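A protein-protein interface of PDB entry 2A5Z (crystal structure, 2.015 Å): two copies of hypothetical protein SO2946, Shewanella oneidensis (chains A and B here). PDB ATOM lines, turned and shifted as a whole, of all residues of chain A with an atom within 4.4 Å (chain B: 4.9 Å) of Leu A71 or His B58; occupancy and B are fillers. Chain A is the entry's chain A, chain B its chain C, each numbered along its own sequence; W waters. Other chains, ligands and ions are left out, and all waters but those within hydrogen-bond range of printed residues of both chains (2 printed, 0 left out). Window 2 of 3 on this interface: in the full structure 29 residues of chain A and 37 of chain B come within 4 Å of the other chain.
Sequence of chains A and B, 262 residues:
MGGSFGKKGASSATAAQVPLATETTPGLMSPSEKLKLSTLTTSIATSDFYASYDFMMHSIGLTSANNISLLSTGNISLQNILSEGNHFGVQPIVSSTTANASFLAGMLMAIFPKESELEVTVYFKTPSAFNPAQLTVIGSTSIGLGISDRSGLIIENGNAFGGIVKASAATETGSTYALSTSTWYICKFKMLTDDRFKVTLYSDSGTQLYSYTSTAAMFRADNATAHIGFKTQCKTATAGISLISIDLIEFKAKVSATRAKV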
ATOM      1  N   SER A  69      16.162 -14.874 -23.412  1.00  0.00           N
ATOM      2  CA  SER A  69      14.902 -14.159 -23.623  1.00  0.00           C
ATOM      3  C   SER A  69      13.730 -15.095 -23.351  1.00  0.00           C
ATOM      4  O   SER A  69      13.761 -16.278 -23.740  1.00  0.00           O
ATOM      5  CB  SER A  69      14.815 -13.614 -25.053  1.00  0.00           C
ATOM      6  OG  SER A  69      16.007 -12.927 -25.424  1.00  0.00           O
ATOM      7  N   LEU A  70      12.712 -14.570 -22.668  1.00  0.00           N
ATOM      8  CA  LEU A  70      11.493 -15.328 -22.349  1.00  0.00           C
ATOM      9  C   LEU A  70      10.325 -14.504 -22.856  1.00  0.00           C
ATOM     10  O   LEU A  70       9.799 -13.620 -22.161  1.00  0.00           O
ATOM     11  CB  LEU A  70      11.385 -15.626 -20.843  1.00  0.00           C
ATOM     12  CG  LEU A  70      12.543 -16.391 -20.186  1.00  0.00           C
ATOM     13  CD1 LEU A  70      12.372 -16.429 -18.676  1.00  0.00           C
ATOM     14  CD2 LEU A  70      12.674 -17.810 -20.758  1.00  0.00           C
ATOM     15  N   LEU A  71       9.958 -14.778 -24.101  1.00  0.00           N
ATOM     16  CA  LEU A  71       9.123 -13.871 -24.871  1.00  0.00           C
ATOM     17  C   LEU A  71       7.728 -14.429 -25.079  1.00  0.00           C
ATOM     18  O   LEU A  71       7.557 -15.482 -25.680  1.00  0.00           O
ATOM     19  CB  LEU A  71       9.780 -13.552 -26.221  1.00  0.00           C
ATOM     20  CG  LEU A  71      11.227 -13.048 -26.204  1.00  0.00           C
ATOM     21  CD1 LEU A  71      11.843 -13.121 -27.605  1.00  0.00           C
ATOM     22  CD2 LEU A  71      11.288 -11.621 -25.659  1.00  0.00           C
ATOM     23  N   SER A  72       6.745 -13.699 -24.570  1.00  0.00           N
ATOM     24  CA  SER A  72       5.344 -14.005 -24.764  1.00  0.00           C
ATOM     25  C   SER A  72       4.781 -13.058 -25.814  1.00  0.00           C
ATOM     26  O   SER A  72       5.073 -11.863 -25.794  1.00  0.00           O
ATOM     27  CB  SER A  72       4.577 -13.813 -23.451  1.00  0.00           C
ATOM     28  OG  SER A  72       4.937 -14.792 -22.489  1.00  0.00           O
ATOM     29  N   THR A  73       3.978 -13.590 -26.728  1.00  0.00           N
ATOM     30  CA  THR A  73       3.266 -12.759 -27.695  1.00  0.00           C
ATOM     31  C   THR A  73       1.845 -13.275 -27.883  1.00  0.00           C
ATOM     32  O   THR A  73       1.541 -14.415 -27.529  1.00  0.00           O
ATOM     33  CB  THR A  73       3.978 -12.708 -29.064  1.00  0.00           C
ATOM     34  OG1 THR A  73       4.168 -14.039 -29.546  1.00  0.00           O
ATOM     35  CG2 THR A  73       5.342 -12.006 -28.963  1.00  0.00           C
ATOM     36  N   SER A 102       2.560 -17.123 -29.113  1.00  0.00           N
ATOM     37  CA  SER A 102       3.708 -17.995 -28.851  1.00  0.00           C
ATOM     38  C   SER A 102       4.461 -17.675 -27.567  1.00  0.00           C
ATOM     39  O   SER A 102       4.386 -16.553 -27.040  1.00  0.00           O
ATOM     40  CB  SER A 102       4.683 -17.955 -30.044  1.00  0.00           C
ATOM     41  OG  SER A 102       5.384 -16.721 -30.102  1.00  0.00           O
ATOM     42  N   PHE A 103       5.168 -18.684 -27.060  1.00  0.00           N
ATOM     43  CA  PHE A 103       6.189 -18.468 -26.052  1.00  0.00           C
ATOM     44  C   PHE A 103       7.539 -18.874 -26.628  1.00  0.00           C
ATOM     45  O   PHE A 103       7.675 -19.966 -27.186  1.00  0.00           O
ATOM     46  CB  PHE A 103       5.904 -19.248 -24.762  1.00  0.00           C
ATOM     47  CG  PHE A 103       6.965 -19.065 -23.708  1.00  0.00           C
ATOM     48  CD1 PHE A 103       7.062 -17.859 -23.002  1.00  0.00           C
ATOM     49  CD2 PHE A 103       7.887 -20.079 -23.445  1.00  0.00           C
ATOM     50  CE1 PHE A 103       8.047 -17.677 -22.042  1.00  0.00           C
ATOM     51  CE2 PHE A 103       8.882 -19.911 -22.488  1.00  0.00           C
ATOM     52  CZ  PHE A 103       8.961 -18.701 -21.782  1.00  0.00           C
ATOM     53  N   LEU A 104       8.527 -17.987 -26.496  1.00  0.00           N
ATOM     54  CA  LEU A 104       9.869 -18.260 -26.998  1.00  0.00           C
ATOM     55  C   LEU A 104      10.900 -18.103 -25.886  1.00  0.00           C
ATOM     56  O   LEU A 104      10.980 -17.053 -25.240  1.00  0.00           O
ATOM     57  CB  LEU A 104      10.207 -17.357 -28.209  1.00  0.00           C
ATOM     58  CG  LEU A 104      11.421 -17.691 -29.092  1.00  0.00           C
ATOM     59  CD1 LEU A 104      11.288 -17.062 -30.473  1.00  0.00           C
ATOM     60  CD2 LEU A 104      12.733 -17.232 -28.437  1.00  0.00           C
ATOM     61  N   LEU A 108      19.732 -14.379 -29.245  1.00  0.00           N
ATOM     62  CA  LEU A 108      19.985 -13.784 -30.558  1.00  0.00           C
ATOM     63  C   LEU A 108      21.050 -14.563 -31.323  1.00  0.00           C
ATOM     64  O   LEU A 108      22.019 -15.029 -30.731  1.00  0.00           O
ATOM     65  CB  LEU A 108      20.438 -12.335 -30.382  1.00  0.00           C
ATOM     66  CG  LEU A 108      19.405 -11.336 -29.867  1.00  0.00           C
ATOM     67  CD1 LEU A 108      20.115 -10.090 -29.380  1.00  0.00           C
ATOM     68  CD2 LEU A 108      18.410 -10.994 -30.953  1.00  0.00           C
ATOM     69  N   ILE A 143      10.669 -14.544 -34.762  1.00  0.00           N
ATOM     70  CA  ILE A 143      10.328 -14.162 -33.396  1.00  0.00           C
ATOM     71  C   ILE A 143       8.820 -13.929 -33.273  1.00  0.00           C
ATOM     72  O   ILE A 143       8.162 -13.604 -34.256  1.00  0.00           O
ATOM     73  CB  ILE A 143      11.134 -12.904 -32.965  1.00  0.00           C
ATOM     74  CG1 ILE A 143      11.327 -12.861 -31.443  1.00  0.00           C
ATOM     75  CG2 ILE A 143      10.514 -11.620 -33.532  1.00  0.00           C
ATOM     76  CD1 ILE A 143      12.217 -11.708 -30.966  1.00  0.00           C
ATOM     77  N   ALA A 224      16.933  -8.815 -34.462  1.00  0.00           N
ATOM     78  CA  ALA A 224      15.847  -9.120 -33.521  1.00  0.00           C
ATOM     79  C   ALA A 224      14.558  -9.685 -34.159  1.00  0.00           C
ATOM     80  O   ALA A 224      13.553  -9.861 -33.466  1.00  0.00           O
ATOM     81  CB  ALA A 224      15.536  -7.901 -32.667  1.00  0.00           C
ATOM     82  N   HIS A 227      15.173 -15.525 -33.344  1.00  0.00           N
ATOM     83  CA  HIS A 227      15.880 -16.028 -32.165  1.00  0.00           C
ATOM     84  C   HIS A 227      16.205 -17.500 -32.420  1.00  0.00           C
ATOM     85  O   HIS A 227      15.618 -18.129 -33.304  1.00  0.00           O
ATOM     86  CB  HIS A 227      15.002 -15.913 -30.914  1.00  0.00           C
ATOM     87  CG  HIS A 227      15.342 -14.762 -30.010  1.00  0.00           C
ATOM     88  ND1 HIS A 227      15.482 -13.467 -30.460  1.00  0.00           N
ATOM     89  CD2 HIS A 227      15.529 -14.713 -28.668  1.00  0.00           C
ATOM     90  CE1 HIS A 227      15.756 -12.673 -29.440  1.00  0.00           C
ATOM     91  NE2 HIS A 227      15.792 -13.403 -28.340  1.00  0.00           N
ATOM     92  N   MET B  56      25.121  -9.006 -24.459  1.00  0.00           N
ATOM     93  CA  MET B  56      24.765 -10.044 -25.430  1.00  0.00           C
ATOM     94  C   MET B  56      23.264 -10.338 -25.474  1.00  0.00           C
ATOM     95  O   MET B  56      22.793 -10.972 -26.416  1.00  0.00           O
ATOM     96  CB  MET B  56      25.574 -11.337 -25.184  1.00  0.00           C
ATOM     97  CG  MET B  56      25.005 -12.270 -24.098  1.00  0.00           C
ATOM     98  SD  MET B  56      25.213 -11.715 -22.389  1.00  0.00           S
ATOM     99  CE  MET B  56      26.865 -12.287 -22.058  1.00  0.00           C
ATOM    100  N   MET B  57      22.524  -9.882 -24.459  1.00  0.00           N
ATOM    101  CA  MET B  57      21.089 -10.174 -24.346  1.00  0.00           C
ATOM    102  C   MET B  57      20.244  -9.328 -25.302  1.00  0.00           C
ATOM    103  O   MET B  57      20.599  -8.190 -25.634  1.00  0.00           O
ATOM    104  CB  MET B  57      20.572  -9.972 -22.909  1.00  0.00           C
ATOM    105  CG  MET B  57      21.319 -10.729 -21.802  1.00  0.00           C
ATOM    106  SD  MET B  57      20.648 -10.387 -20.135  1.00  0.00           S
ATOM    107  CE  MET B  57      18.965 -10.935 -20.398  1.00  0.00           C
ATOM    108  N   HIS B  58      19.137  -9.916 -25.753  1.00  0.00           N
ATOM    109  CA  HIS B  58      18.065  -9.206 -26.456  1.00  0.00           C
ATOM    110  C   HIS B  58      17.663  -8.028 -25.557  1.00  0.00           C
ATOM    111  O   HIS B  58      17.394  -8.224 -24.367  1.00  0.00           O
ATOM    112  CB  HIS B  58      16.910 -10.197 -26.658  1.00  0.00           C
ATOM    113  CG  HIS B  58      15.743  -9.667 -27.435  1.00  0.00           C
ATOM    114  ND1 HIS B  58      15.863  -9.127 -28.698  1.00  0.00           N
ATOM    115  CD2 HIS B  58      14.418  -9.661 -27.148  1.00  0.00           C
ATOM    116  CE1 HIS B  58      14.664  -8.787 -29.145  1.00  0.00           C
ATOM    117  NE2 HIS B  58      13.770  -9.107 -28.225  1.00  0.00           N
ATOM    118  N   SER B  59      17.668  -6.807 -26.097  1.00  0.00           N
ATOM    119  CA  SER B  59      17.555  -5.624 -25.226  1.00  0.00           C
ATOM    120  C   SER B  59      16.189  -4.936 -25.160  1.00  0.00           C
ATOM    121  O   SER B  59      16.040  -3.945 -24.438  1.00  0.00           O
ATOM    122  CB  SER B  59      18.679  -4.608 -25.484  1.00  0.00           C
ATOM    123  OG  SER B  59      18.687  -4.135 -26.821  1.00  0.00           O
ATOM    124  N   ILE B  60      15.197  -5.467 -25.881  1.00  0.00           N
ATOM    125  CA  ILE B  60      13.813  -4.981 -25.756  1.00  0.00           C
ATOM    126  C   ILE B  60      13.290  -5.234 -24.348  1.00  0.00           C
ATOM    127  O   ILE B  60      13.197  -6.389 -23.912  1.00  0.00           O
ATOM    128  CB  ILE B  60      12.844  -5.670 -26.743  1.00  0.00           C
ATOM    129  CG1 ILE B  60      13.344  -5.553 -28.190  1.00  0.00           C
ATOM    130  CG2 ILE B  60      11.406  -5.127 -26.557  1.00  0.00           C
ATOM    131  CD1 ILE B  60      12.768  -4.402 -28.997  1.00  0.00           C
ATOM    132  N   LEU B  62      14.687  -4.601 -21.530  1.00  0.00           N
ATOM    133  CA  LEU B  62      15.743  -5.055 -20.619  1.00  0.00           C
ATOM    134  C   LEU B  62      16.236  -3.880 -19.782  1.00  0.00           C
ATOM    135  O   LEU B  62      16.952  -3.008 -20.280  1.00  0.00           O
ATOM    136  CB  LEU B  62      16.914  -5.671 -21.399  1.00  0.00           C
ATOM    137  CG  LEU B  62      18.106  -6.234 -20.603  1.00  0.00           C
ATOM    138  CD1 LEU B  62      17.694  -7.459 -19.797  1.00  0.00           C
ATOM    139  CD2 LEU B  62      19.266  -6.576 -21.535  1.00  0.00           C
HETATM  140  O   HOH W   1      18.629 -12.814 -24.757  1.00  0.00           O
HETATM  141  O   HOH W   2      20.621 -12.972 -26.857  1.00  0.00           O
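Ser A69 touches His B58 (OG to CB, 3.1 Å).
CD2 of Leu A71 touches CD2 of His B58, 3.98 Å away.
CA of His B58 touches CD1 of Leu A108, at 3.7 Å.
Ala A224 touches His B58.
CE1 of His A227 touches CG of His B58 (3.6 Å).
A ring nitrogen (NE2) of His A227 sits at hydrogen-bond distance from the side-chain hydroxyl of Ser A69, at 3.0 Å.
The backbone NH (N) of Leu A71 lies within hydrogen-bond range of the backbone carbonyl oxygen (O) of Leu A104, 2.7 Å away.
No position is printed for both chains.
Of the 5 pairs that touch across the chains among the printed residues, none has its exchanged pair printed and touching as well.
Printed residues of chain B within 4 Å of Leu A71: His B58.
Printed residues of chain A within 4 Å of His B58: Ser A69 (3.1 Å), Leu A71 (3.98 Å), Leu A108 (3.7 Å), Ala A224 (3.7 Å) and His A227 (3.6 Å).
Printed residues of chain B within 4 Å of Leu A108: His B58.
Of the printed residues of chain B, His A227 touches His B58.
Printed residues of chain B within 4 Å of Ala A224: His B58.
Leu A104 touches none of the printed residues of chain B.
The nearest printed residue of chain B that does not touch Leu A71 is Ile B60 (5.8 Å).
The nearest printed residue of chain A that does not touch His B58 is Ile A143 (4.1 Å).
The nearest printed residue of chain B that does not touch Leu A108 is Met B56 (4.1 Å).
Printed residues of chain B that touch a printed residue of chain A: His B58.
Hydrophobic or aromatic side chains of chain A that line the printed part of chain B: Leu A71, Leu A108, Ala A224 and His A227.
Among the printed residues, 5 pairs touch across the chains.
Among the printed residues, no Asp or Glu carboxylate lies within 4 Å of a Lys or Arg side-chain nitrogen of the other chain.
Water W1 bridges the side-chain hydroxyl of Ser A69 (2.7 Å) and the backbone NH of His B58 (3.1 Å).
Water W2 bridges the backbone NH of Leu A108 (2.9 Å) and the backbone carbonyl oxygen of Met B56 (3.0 Å).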
